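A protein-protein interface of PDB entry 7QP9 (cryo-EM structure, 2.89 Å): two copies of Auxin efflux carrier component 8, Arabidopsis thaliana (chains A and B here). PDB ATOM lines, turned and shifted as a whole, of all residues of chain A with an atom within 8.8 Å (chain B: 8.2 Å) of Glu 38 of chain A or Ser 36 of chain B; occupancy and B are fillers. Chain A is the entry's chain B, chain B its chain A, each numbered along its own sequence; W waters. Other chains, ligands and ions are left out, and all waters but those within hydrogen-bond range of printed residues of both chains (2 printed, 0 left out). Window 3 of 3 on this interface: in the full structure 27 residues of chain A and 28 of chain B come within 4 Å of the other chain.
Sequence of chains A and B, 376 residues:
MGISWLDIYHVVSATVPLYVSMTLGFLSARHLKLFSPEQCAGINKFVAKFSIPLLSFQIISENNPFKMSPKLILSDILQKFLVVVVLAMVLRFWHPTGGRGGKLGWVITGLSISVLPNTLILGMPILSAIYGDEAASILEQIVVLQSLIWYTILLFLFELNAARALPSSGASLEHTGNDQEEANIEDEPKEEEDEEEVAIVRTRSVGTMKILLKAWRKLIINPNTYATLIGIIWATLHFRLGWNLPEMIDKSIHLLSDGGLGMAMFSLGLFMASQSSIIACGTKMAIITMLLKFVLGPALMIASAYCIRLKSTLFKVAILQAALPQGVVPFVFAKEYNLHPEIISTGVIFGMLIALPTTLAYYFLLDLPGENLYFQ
Among the printed residues, pairs that only touch across the chains: Phe 35 of chain A with Gly 42 of chain B (3.3 Å), Ser 36 of chain A with Glu 38 of chain B (3.5 Å), Glu 38 of chain A with Ser 36 of chain B (3.5 Å), Glu 38 of chain A with Glu 38 of chain B (3.9 Å), Gln 39 of chain A with Ala 41 of chain B (3.98 Å), Ala 41 of chain A with Gln 39 of chain B (3.97 Å), Gly 42 of chain A with Phe 35 of chain B (3.3 Å) and Lys 45 of chain A with Gln 39 of chain B (3.97 Å).
The backbone carbonyl oxygen of Ser 28 of chain B lies within hydrogen-bond range of the backbone NH of Leu 34 of chain B, at 2.7 Å. The backbone carbonyl oxygen (O) of Leu 34 of chain B sits close to the side-chain amide oxygen (OE1) of Gln 39 of chain B. The backbone carbonyl oxygen (O) of Ser 36 of chain B lies within hydrogen-bond range of the side-chain sulfur (SG) of Cys 40 of chain B (3.4 Å). The side-chain sulfur of Cys 40 of chain A sits at hydrogen-bond distance from the backbone carbonyl oxygen of Ser 36 of chain A (3.4 Å). The side-chain carboxylate (OE2) of Glu 336 of chain A lies close to the backbone NH (N) of Lys 45 of chain A (3.4 Å).
Glu 38 of chain A touches just these residues of chain B: Ser 36, Glu 38 and Gln 39. Of the printed residues of chain B, Gly 42 of chain A touches Phe 35 (3.3 Å) and Gln 39 (3.5 Å). Lys 33 of chain B touches none of the printed residues of chain A. No residue of chain A comes within 4 Å of Pro 37 of chain B. Printed residues of chain A within 4 Å of Glu 38 of chain B: Ser 36 (3.5 Å), Glu 38 (3.9 Å) and Gln 39 (3.4 Å). Of the printed residues of chain A, Ala 41 of chain B touches Gln 39 (3.98 Å). Of the printed residues of chain A, Gly 42 of chain B touches Phe 35 (3.3 Å) and Gln 39 (3.5 Å). The nearest printed residue of chain B that does not touch Glu 38 of chain A is Pro 37 of chain B (6.9 Å). The nearest residue of chain A that does not touch Ser 36 of chain B is Lys 45 of chain A (5.9 Å).
Water W1 lies within hydrogen-bond range of the backbone carbonyl oxygen of Leu 34 of chain B (3.2 Å) and the side-chain amino group of Lys 45 of chain A (3.3 Å). Water W2 bridges the side-chain amide nitrogen (NE2) of Gln 39 of chain B and the side-chain amino group (NZ) of Lys 45 of chain A.
Hydrophobic or aromatic side chains of chain A that line the printed part of chain B: Phe 35 and Ala 41. Along chain A the printed residues that touch a printed residue of chain B span positions 35 to 45. Of the 15 printed residues of chain B, 7 touch a printed residue of chain A. Hydrophobic or aromatic side chains of chain B within 4 Å of the printed part of chain A: Phe 35 and Ala 41. Among the printed residues, 13 pairs touch across the chains. Among the printed residues, no Asp or Glu carboxylate lies within 4 Å of a Lys or Arg side-chain nitrogen of the other chain.
Glu 38 of chain B touches its own counterpart, Glu 38 of chain A. Glu 38 of chain A touches Gln 39 of chain B, and with the chains exchanged Gln 39 of chain A touches Glu 38 of chain B. Gln 39 of chain A touches Ala 41 of chain B, and with the chains exchanged Ala 41 of chain A touches Gln 39 of chain B. Gln 39 of chain A touches Gly 42 of chain B, and with the chains exchanged Gly 42 of chain A touches Gln 39 of chain B.
O of Leu 34 of chain B lies within hydrogen-bond range of NZ of Lys 45 of chain A, at 2.4 Å. NE2 of Gln 39 of chain A lies within hydrogen-bond range of O of Glu 38 of chain B, 3.4 Å away. The backbone carbonyl oxygen of Glu 38 of chain A sits at hydrogen-bond distance from the side-chain amide nitrogen of Gln 39 of chain B (3.4 Å). NE2 of Gln 39 of chain B lies close to N of Gly 42 of chain A, at 3.5 Å. The backbone NH (N) of Gly 42 of chain B lies close to the side-chain amide nitrogen (NE2) of Gln 39 of chain A, 3.5 Å away.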
ATOM      1  N   PHE A  35     -15.601  26.461  16.043  1.00  0.00           N
ATOM      2  CA  PHE A  35     -16.699  26.587  16.989  1.00  0.00           C
ATOM      3  C   PHE A  35     -17.012  28.054  17.237  1.00  0.00           C
ATOM      4  O   PHE A  35     -16.105  28.855  17.482  1.00  0.00           O
ATOM      5  CB  PHE A  35     -16.361  25.894  18.310  1.00  0.00           C
ATOM      6  CG  PHE A  35     -16.004  24.449  18.156  1.00  0.00           C
ATOM      7  CD1 PHE A  35     -16.980  23.508  17.893  1.00  0.00           C
ATOM      8  CD2 PHE A  35     -14.692  24.032  18.268  1.00  0.00           C
ATOM      9  CE1 PHE A  35     -16.653  22.179  17.749  1.00  0.00           C
ATOM     10  CE2 PHE A  35     -14.362  22.704  18.124  1.00  0.00           C
ATOM     11  CZ  PHE A  35     -15.342  21.777  17.863  1.00  0.00           C
ATOM     12  N   SER A  36     -18.289  28.396  17.168  1.00  0.00           N
ATOM     13  CA  SER A  36     -18.774  29.714  17.547  1.00  0.00           C
ATOM     14  C   SER A  36     -19.027  29.757  19.044  1.00  0.00           C
ATOM     15  O   SER A  36     -19.074  28.723  19.712  1.00  0.00           O
ATOM     16  CB  SER A  36     -20.042  30.039  16.765  1.00  0.00           C
ATOM     17  OG  SER A  36     -21.145  29.298  17.250  1.00  0.00           O
ATOM     18  N   PRO A  37     -19.191  30.950  19.617  1.00  0.00           N
ATOM     19  CA  PRO A  37     -19.391  31.032  21.074  1.00  0.00           C
ATOM     20  C   PRO A  37     -20.542  30.177  21.580  1.00  0.00           C
ATOM     21  O   PRO A  37     -20.434  29.577  22.655  1.00  0.00           O
ATOM     22  CB  PRO A  37     -19.647  32.527  21.302  1.00  0.00           C
ATOM     23  CG  PRO A  37     -18.980  33.203  20.162  1.00  0.00           C
ATOM     24  CD  PRO A  37     -19.127  32.283  18.992  1.00  0.00           C
ATOM     25  N   GLU A  38     -21.644  30.103  20.830  1.00  0.00           N
ATOM     26  CA  GLU A  38     -22.754  29.247  21.235  1.00  0.00           C
ATOM     27  C   GLU A  38     -22.338  27.782  21.261  1.00  0.00           C
ATOM     28  O   GLU A  38     -22.696  27.042  22.183  1.00  0.00           O
ATOM     29  CB  GLU A  38     -23.938  29.451  20.291  1.00  0.00           C
ATOM     30  CG  GLU A  38     -25.213  28.733  20.711  1.00  0.00           C
ATOM     31  CD  GLU A  38     -26.035  29.531  21.700  1.00  0.00           C
ATOM     32  OE1 GLU A  38     -25.452  30.364  22.427  1.00  0.00           O
ATOM     33  OE2 GLU A  38     -27.266  29.327  21.752  1.00  0.00           O
ATOM     34  N   GLN A  39     -21.581  27.343  20.255  1.00  0.00           N
ATOM     35  CA  GLN A  39     -21.141  25.953  20.213  1.00  0.00           C
ATOM     36  C   GLN A  39     -20.140  25.655  21.323  1.00  0.00           C
ATOM     37  O   GLN A  39     -20.151  24.562  21.901  1.00  0.00           O
ATOM     38  CB  GLN A  39     -20.544  25.646  18.843  1.00  0.00           C
ATOM     39  CG  GLN A  39     -21.499  25.934  17.698  1.00  0.00           C
ATOM     40  CD  GLN A  39     -20.997  25.414  16.370  1.00  0.00           C
ATOM     41  OE1 GLN A  39     -19.794  25.330  16.140  1.00  0.00           O
ATOM     42  NE2 GLN A  39     -21.921  25.067  15.485  1.00  0.00           N
ATOM     43  N   CYS A  40     -19.264  26.612  21.636  1.00  0.00           N
ATOM     44  CA  CYS A  40     -18.358  26.440  22.767  1.00  0.00           C
ATOM     45  C   CYS A  40     -19.136  26.322  24.072  1.00  0.00           C
ATOM     46  O   CYS A  40     -18.813  25.487  24.927  1.00  0.00           O
ATOM     47  CB  CYS A  40     -17.376  27.608  22.832  1.00  0.00           C
ATOM     48  SG  CYS A  40     -16.279  27.744  21.404  1.00  0.00           S
ATOM     49  N   ALA A  41     -20.165  27.153  24.241  1.00  0.00           N
ATOM     50  CA  ALA A  41     -21.007  27.056  25.426  1.00  0.00           C
ATOM     51  C   ALA A  41     -21.708  25.708  25.486  1.00  0.00           C
ATOM     52  O   ALA A  41     -21.863  25.130  26.565  1.00  0.00           O
ATOM     53  CB  ALA A  41     -22.028  28.193  25.438  1.00  0.00           C
ATOM     54  N   GLY A  42     -22.148  25.195  24.338  1.00  0.00           N
ATOM     55  CA  GLY A  42     -22.773  23.882  24.317  1.00  0.00           C
ATOM     56  C   GLY A  42     -21.818  22.772  24.709  1.00  0.00           C
ATOM     57  O   GLY A  42     -22.186  21.852  25.444  1.00  0.00           O
ATOM     58  N   ILE A  43     -20.580  22.836  24.219  1.00  0.00           N
ATOM     59  CA  ILE A  43     -19.581  21.840  24.600  1.00  0.00           C
ATOM     60  C   ILE A  43     -19.315  21.906  26.099  1.00  0.00           C
ATOM     61  O   ILE A  43     -19.237  20.873  26.781  1.00  0.00           O
ATOM     62  CB  ILE A  43     -18.291  22.040  23.783  1.00  0.00           C
ATOM     63  CG1 ILE A  43     -18.439  21.414  22.396  1.00  0.00           C
ATOM     64  CG2 ILE A  43     -17.093  21.432  24.502  1.00  0.00           C
ATOM     65  CD1 ILE A  43     -17.589  22.071  21.341  1.00  0.00           C
ATOM     66  N   ASN A  44     -19.170  23.118  26.639  1.00  0.00           N
ATOM     67  CA  ASN A  44     -18.944  23.258  28.073  1.00  0.00           C
ATOM     68  C   ASN A  44     -20.135  22.741  28.870  1.00  0.00           C
ATOM     69  O   ASN A  44     -19.963  22.126  29.927  1.00  0.00           O
ATOM     70  CB  ASN A  44     -18.661  24.718  28.423  1.00  0.00           C
ATOM     71  CG  ASN A  44     -18.013  24.874  29.784  1.00  0.00           C
ATOM     72  OD1 ASN A  44     -16.800  24.737  29.925  1.00  0.00           O
ATOM     73  ND2 ASN A  44     -18.823  25.160  30.795  1.00  0.00           N
ATOM     74  N   LYS A  45     -21.354  22.993  28.389  1.00  0.00           N
ATOM     75  CA  LYS A  45     -22.540  22.497  29.075  1.00  0.00           C
ATOM     76  C   LYS A  45     -22.581  20.977  29.067  1.00  0.00           C
ATOM     77  O   LYS A  45     -22.956  20.355  30.065  1.00  0.00           O
ATOM     78  CB  LYS A  45     -23.799  23.065  28.422  1.00  0.00           C
ATOM     79  CG  LYS A  45     -25.082  22.727  29.161  1.00  0.00           C
ATOM     80  CD  LYS A  45     -26.304  23.089  28.344  1.00  0.00           C
ATOM     81  CE  LYS A  45     -26.603  24.572  28.414  1.00  0.00           C
ATOM     82  NZ  LYS A  45     -27.945  24.890  27.852  1.00  0.00           N
ATOM     83  N   LEU A 270     -11.172  26.494  24.489  1.00  0.00           N
ATOM     84  CA  LEU A 270     -12.181  27.230  23.735  1.00  0.00           C
ATOM     85  C   LEU A 270     -12.482  28.568  24.394  1.00  0.00           C
ATOM     86  O   LEU A 270     -12.626  29.588  23.712  1.00  0.00           O
ATOM     87  CB  LEU A 270     -13.460  26.401  23.614  1.00  0.00           C
ATOM     88  CG  LEU A 270     -13.430  25.147  22.739  1.00  0.00           C
ATOM     89  CD1 LEU A 270     -14.703  24.345  22.929  1.00  0.00           C
ATOM     90  CD2 LEU A 270     -13.250  25.500  21.281  1.00  0.00           C
ATOM     91  N   LYS A 335     -17.569  28.755  34.122  1.00  0.00           N
ATOM     92  CA  LYS A 335     -18.010  29.051  32.764  1.00  0.00           C
ATOM     93  C   LYS A 335     -19.508  28.825  32.614  1.00  0.00           C
ATOM     94  O   LYS A 335     -20.203  29.627  31.982  1.00  0.00           O
ATOM     95  CB  LYS A 335     -17.230  28.189  31.770  1.00  0.00           C
ATOM     96  CG  LYS A 335     -17.613  28.385  30.310  1.00  0.00           C
ATOM     97  CD  LYS A 335     -17.032  29.664  29.745  1.00  0.00           C
ATOM     98  CE  LYS A 335     -17.906  30.222  28.634  1.00  0.00           C
ATOM     99  NZ  LYS A 335     -18.087  29.248  27.524  1.00  0.00           N
ATOM    100  N   GLU A 336     -20.026  27.736  33.188  1.00  0.00           N
ATOM    101  CA  GLU A 336     -21.459  27.482  33.110  1.00  0.00           C
ATOM    102  C   GLU A 336     -22.253  28.598  33.774  1.00  0.00           C
ATOM    103  O   GLU A 336     -23.266  29.055  33.235  1.00  0.00           O
ATOM    104  CB  GLU A 336     -21.789  26.136  33.755  1.00  0.00           C
ATOM    105  CG  GLU A 336     -21.717  24.945  32.812  1.00  0.00           C
ATOM    106  CD  GLU A 336     -22.596  25.108  31.587  1.00  0.00           C
ATOM    107  OE1 GLU A 336     -23.799  24.781  31.671  1.00  0.00           O
ATOM    108  OE2 GLU A 336     -22.087  25.568  30.543  1.00  0.00           O
ATOM    109  N   SER B  28     -31.870  15.022  26.324  1.00  0.00           N
ATOM    110  CA  SER B  28     -31.243  16.318  26.550  1.00  0.00           C
ATOM    111  C   SER B  28     -31.719  17.343  25.532  1.00  0.00           C
ATOM    112  O   SER B  28     -32.008  18.493  25.885  1.00  0.00           O
ATOM    113  CB  SER B  28     -29.726  16.175  26.488  1.00  0.00           C
ATOM    114  OG  SER B  28     -29.293  15.134  27.341  1.00  0.00           O
ATOM    115  N   ALA B  29     -31.802  16.952  24.263  1.00  0.00           N
ATOM    116  CA  ALA B  29     -32.192  17.908  23.234  1.00  0.00           C
ATOM    117  C   ALA B  29     -33.689  18.195  23.253  1.00  0.00           C
ATOM    118  O   ALA B  29     -34.102  19.336  23.022  1.00  0.00           O
ATOM    119  CB  ALA B  29     -31.769  17.402  21.858  1.00  0.00           C
ATOM    120  N   LYS B  33     -34.025  19.915  27.052  1.00  0.00           N
ATOM    121  CA  LYS B  33     -33.758  21.096  26.233  1.00  0.00           C
ATOM    122  C   LYS B  33     -32.451  21.763  26.648  1.00  0.00           C
ATOM    123  O   LYS B  33     -32.337  22.989  26.675  1.00  0.00           O
ATOM    124  CB  LYS B  33     -34.922  22.084  26.307  1.00  0.00           C
ATOM    125  CG  LYS B  33     -36.197  21.564  25.671  1.00  0.00           C
ATOM    126  CD  LYS B  33     -37.308  22.593  25.719  1.00  0.00           C
ATOM    127  CE  LYS B  33     -38.600  22.030  25.151  1.00  0.00           C
ATOM    128  NZ  LYS B  33     -38.501  21.772  23.688  1.00  0.00           N
ATOM    129  N   LEU B  34     -31.451  20.942  26.976  1.00  0.00           N
ATOM    130  CA  LEU B  34     -30.157  21.480  27.381  1.00  0.00           C
ATOM    131  C   LEU B  34     -29.433  22.128  26.210  1.00  0.00           C
ATOM    132  O   LEU B  34     -28.738  23.135  26.384  1.00  0.00           O
ATOM    133  CB  LEU B  34     -29.297  20.372  27.987  1.00  0.00           C
ATOM    134  CG  LEU B  34     -29.771  19.801  29.321  1.00  0.00           C
ATOM    135  CD1 LEU B  34     -29.075  18.489  29.607  1.00  0.00           C
ATOM    136  CD2 LEU B  34     -29.527  20.791  30.444  1.00  0.00           C
ATOM    137  N   PHE B  35     -29.583  21.570  25.011  1.00  0.00           N
ATOM    138  CA  PHE B  35     -28.812  21.982  23.846  1.00  0.00           C
ATOM    139  C   PHE B  35     -29.736  22.548  22.780  1.00  0.00           C
ATOM    140  O   PHE B  35     -30.768  21.948  22.463  1.00  0.00           O
ATOM    141  CB  PHE B  35     -28.016  20.806  23.278  1.00  0.00           C
ATOM    142  CG  PHE B  35     -27.102  20.161  24.273  1.00  0.00           C
ATOM    143  CD1 PHE B  35     -25.936  20.788  24.664  1.00  0.00           C
ATOM    144  CD2 PHE B  35     -27.414  18.934  24.823  1.00  0.00           C
ATOM    145  CE1 PHE B  35     -25.096  20.200  25.581  1.00  0.00           C
ATOM    146  CE2 PHE B  35     -26.577  18.342  25.741  1.00  0.00           C
ATOM    147  CZ  PHE B  35     -25.417  18.975  26.121  1.00  0.00           C
ATOM    148  N   SER B  36     -29.363  23.697  22.239  1.00  0.00           N
ATOM    149  CA  SER B  36     -30.040  24.286  21.094  1.00  0.00           C
ATOM    150  C   SER B  36     -29.461  23.720  19.810  1.00  0.00           C
ATOM    151  O   SER B  36     -28.400  23.094  19.810  1.00  0.00           O
ATOM    152  CB  SER B  36     -29.899  25.804  21.139  1.00  0.00           C
ATOM    153  OG  SER B  36     -28.588  26.206  20.791  1.00  0.00           O
ATOM    154  N   PRO B  37     -30.141  23.914  18.677  1.00  0.00           N
ATOM    155  CA  PRO B  37     -29.635  23.333  17.422  1.00  0.00           C
ATOM    156  C   PRO B  37     -28.199  23.720  17.107  1.00  0.00           C
ATOM    157  O   PRO B  37     -27.434  22.886  16.608  1.00  0.00           O
ATOM    158  CB  PRO B  37     -30.616  23.875  16.374  1.00  0.00           C
ATOM    159  CG  PRO B  37     -31.863  24.149  17.130  1.00  0.00           C
ATOM    160  CD  PRO B  37     -31.432  24.597  18.491  1.00  0.00           C
ATOM    161  N   GLU B  38     -27.809  24.965  17.385  1.00  0.00           N
ATOM    162  CA  GLU B  38     -26.426  25.372  17.164  1.00  0.00           C
ATOM    163  C   GLU B  38     -25.472  24.579  18.047  1.00  0.00           C
ATOM    164  O   GLU B  38     -24.404  24.151  17.595  1.00  0.00           O
ATOM    165  CB  GLU B  38     -26.276  26.870  17.425  1.00  0.00           C
ATOM    166  CG  GLU B  38     -24.913  27.441  17.062  1.00  0.00           C
ATOM    167  CD  GLU B  38     -24.809  27.823  15.601  1.00  0.00           C
ATOM    168  OE1 GLU B  38     -25.537  27.233  14.777  1.00  0.00           O
ATOM    169  OE2 GLU B  38     -23.996  28.713  15.277  1.00  0.00           O
ATOM    170  N   GLN B  39     -25.838  24.371  19.312  1.00  0.00           N
ATOM    171  CA  GLN B  39     -24.978  23.616  20.216  1.00  0.00           C
ATOM    172  C   GLN B  39     -24.903  22.147  19.816  1.00  0.00           C
ATOM    173  O   GLN B  39     -23.846  21.518  19.933  1.00  0.00           O
ATOM    174  CB  GLN B  39     -25.482  23.768  21.648  1.00  0.00           C
ATOM    175  CG  GLN B  39     -25.587  25.215  22.095  1.00  0.00           C
ATOM    176  CD  GLN B  39     -25.850  25.356  23.576  1.00  0.00           C
ATOM    177  OE1 GLN B  39     -26.471  24.494  24.192  1.00  0.00           O
ATOM    178  NE2 GLN B  39     -25.379  26.451  24.157  1.00  0.00           N
ATOM    179  N   CYS B  40     -26.016  21.581  19.344  1.00  0.00           N
ATOM    180  CA  CYS B  40     -25.985  20.216  18.831  1.00  0.00           C
ATOM    181  C   CYS B  40     -25.072  20.113  17.616  1.00  0.00           C
ATOM    182  O   CYS B  40     -24.304  19.150  17.481  1.00  0.00           O
ATOM    183  CB  CYS B  40     -27.401  19.759  18.477  1.00  0.00           C
ATOM    184  SG  CYS B  40     -28.535  19.684  19.881  1.00  0.00           S
ATOM    185  N   ALA B  41     -25.142  21.097  16.719  1.00  0.00           N
ATOM    186  CA  ALA B  41     -24.249  21.114  15.567  1.00  0.00           C
ATOM    187  C   ALA B  41     -22.797  21.225  16.007  1.00  0.00           C
ATOM    188  O   ALA B  41     -21.914  20.603  15.412  1.00  0.00           O
ATOM    189  CB  ALA B  41     -24.617  22.267  14.636  1.00  0.00           C
ATOM    190  N   GLY B  42     -22.530  22.018  17.044  1.00  0.00           N
ATOM    191  CA  GLY B  42     -21.172  22.121  17.553  1.00  0.00           C
ATOM    192  C   GLY B  42     -20.663  20.816  18.131  1.00  0.00           C
ATOM    193  O   GLY B  42     -19.506  20.440  17.924  1.00  0.00           O
ATOM    194  N   ILE B  43     -21.516  20.107  18.872  1.00  0.00           N
ATOM    195  CA  ILE B  43     -21.124  18.808  19.413  1.00  0.00           C
ATOM    196  C   ILE B  43     -20.831  17.831  18.281  1.00  0.00           C
ATOM    197  O   ILE B  43     -19.834  17.095  18.313  1.00  0.00           O
ATOM    198  CB  ILE B  43     -22.217  18.273  20.358  1.00  0.00           C
ATOM    199  CG1 ILE B  43     -22.106  18.945  21.727  1.00  0.00           C
ATOM    200  CG2 ILE B  43     -22.112  16.762  20.509  1.00  0.00           C
ATOM    201  CD1 ILE B  43     -23.404  18.986  22.491  1.00  0.00           C
ATOM    202  N   LEU B 270     -29.193  13.603  19.754  1.00  0.00           N
ATOM    203  CA  LEU B 270     -29.496  15.026  19.639  1.00  0.00           C
ATOM    204  C   LEU B 270     -30.191  15.330  18.321  1.00  0.00           C
ATOM    205  O   LEU B 270     -31.148  16.110  18.279  1.00  0.00           O
ATOM    206  CB  LEU B 270     -28.214  15.851  19.760  1.00  0.00           C
ATOM    207  CG  LEU B 270     -27.521  15.920  21.123  1.00  0.00           C
ATOM    208  CD1 LEU B 270     -26.167  16.585  20.986  1.00  0.00           C
ATOM    209  CD2 LEU B 270     -28.370  16.661  22.129  1.00  0.00           C
ATOM    210  N   LYS B 335     -24.619  14.328   8.918  1.00  0.00           N
ATOM    211  CA  LYS B 335     -25.064  15.483   9.689  1.00  0.00           C
ATOM    212  C   LYS B 335     -24.154  16.680   9.454  1.00  0.00           C
ATOM    213  O   LYS B 335     -24.629  17.813   9.324  1.00  0.00           O
ATOM    214  CB  LYS B 335     -25.115  15.124  11.174  1.00  0.00           C
ATOM    215  CG  LYS B 335     -25.525  16.262  12.097  1.00  0.00           C
ATOM    216  CD  LYS B 335     -27.004  16.576  11.982  1.00  0.00           C
ATOM    217  CE  LYS B 335     -27.319  17.965  12.512  1.00  0.00           C
ATOM    218  NZ  LYS B 335     -26.646  18.238  13.811  1.00  0.00           N
HETATM  219  O   HOH W   1     -30.381  25.803  25.818  1.00  0.00           O
HETATM  220  O   HOH W   2     -25.768  27.457  27.335  1.00  0.00           O
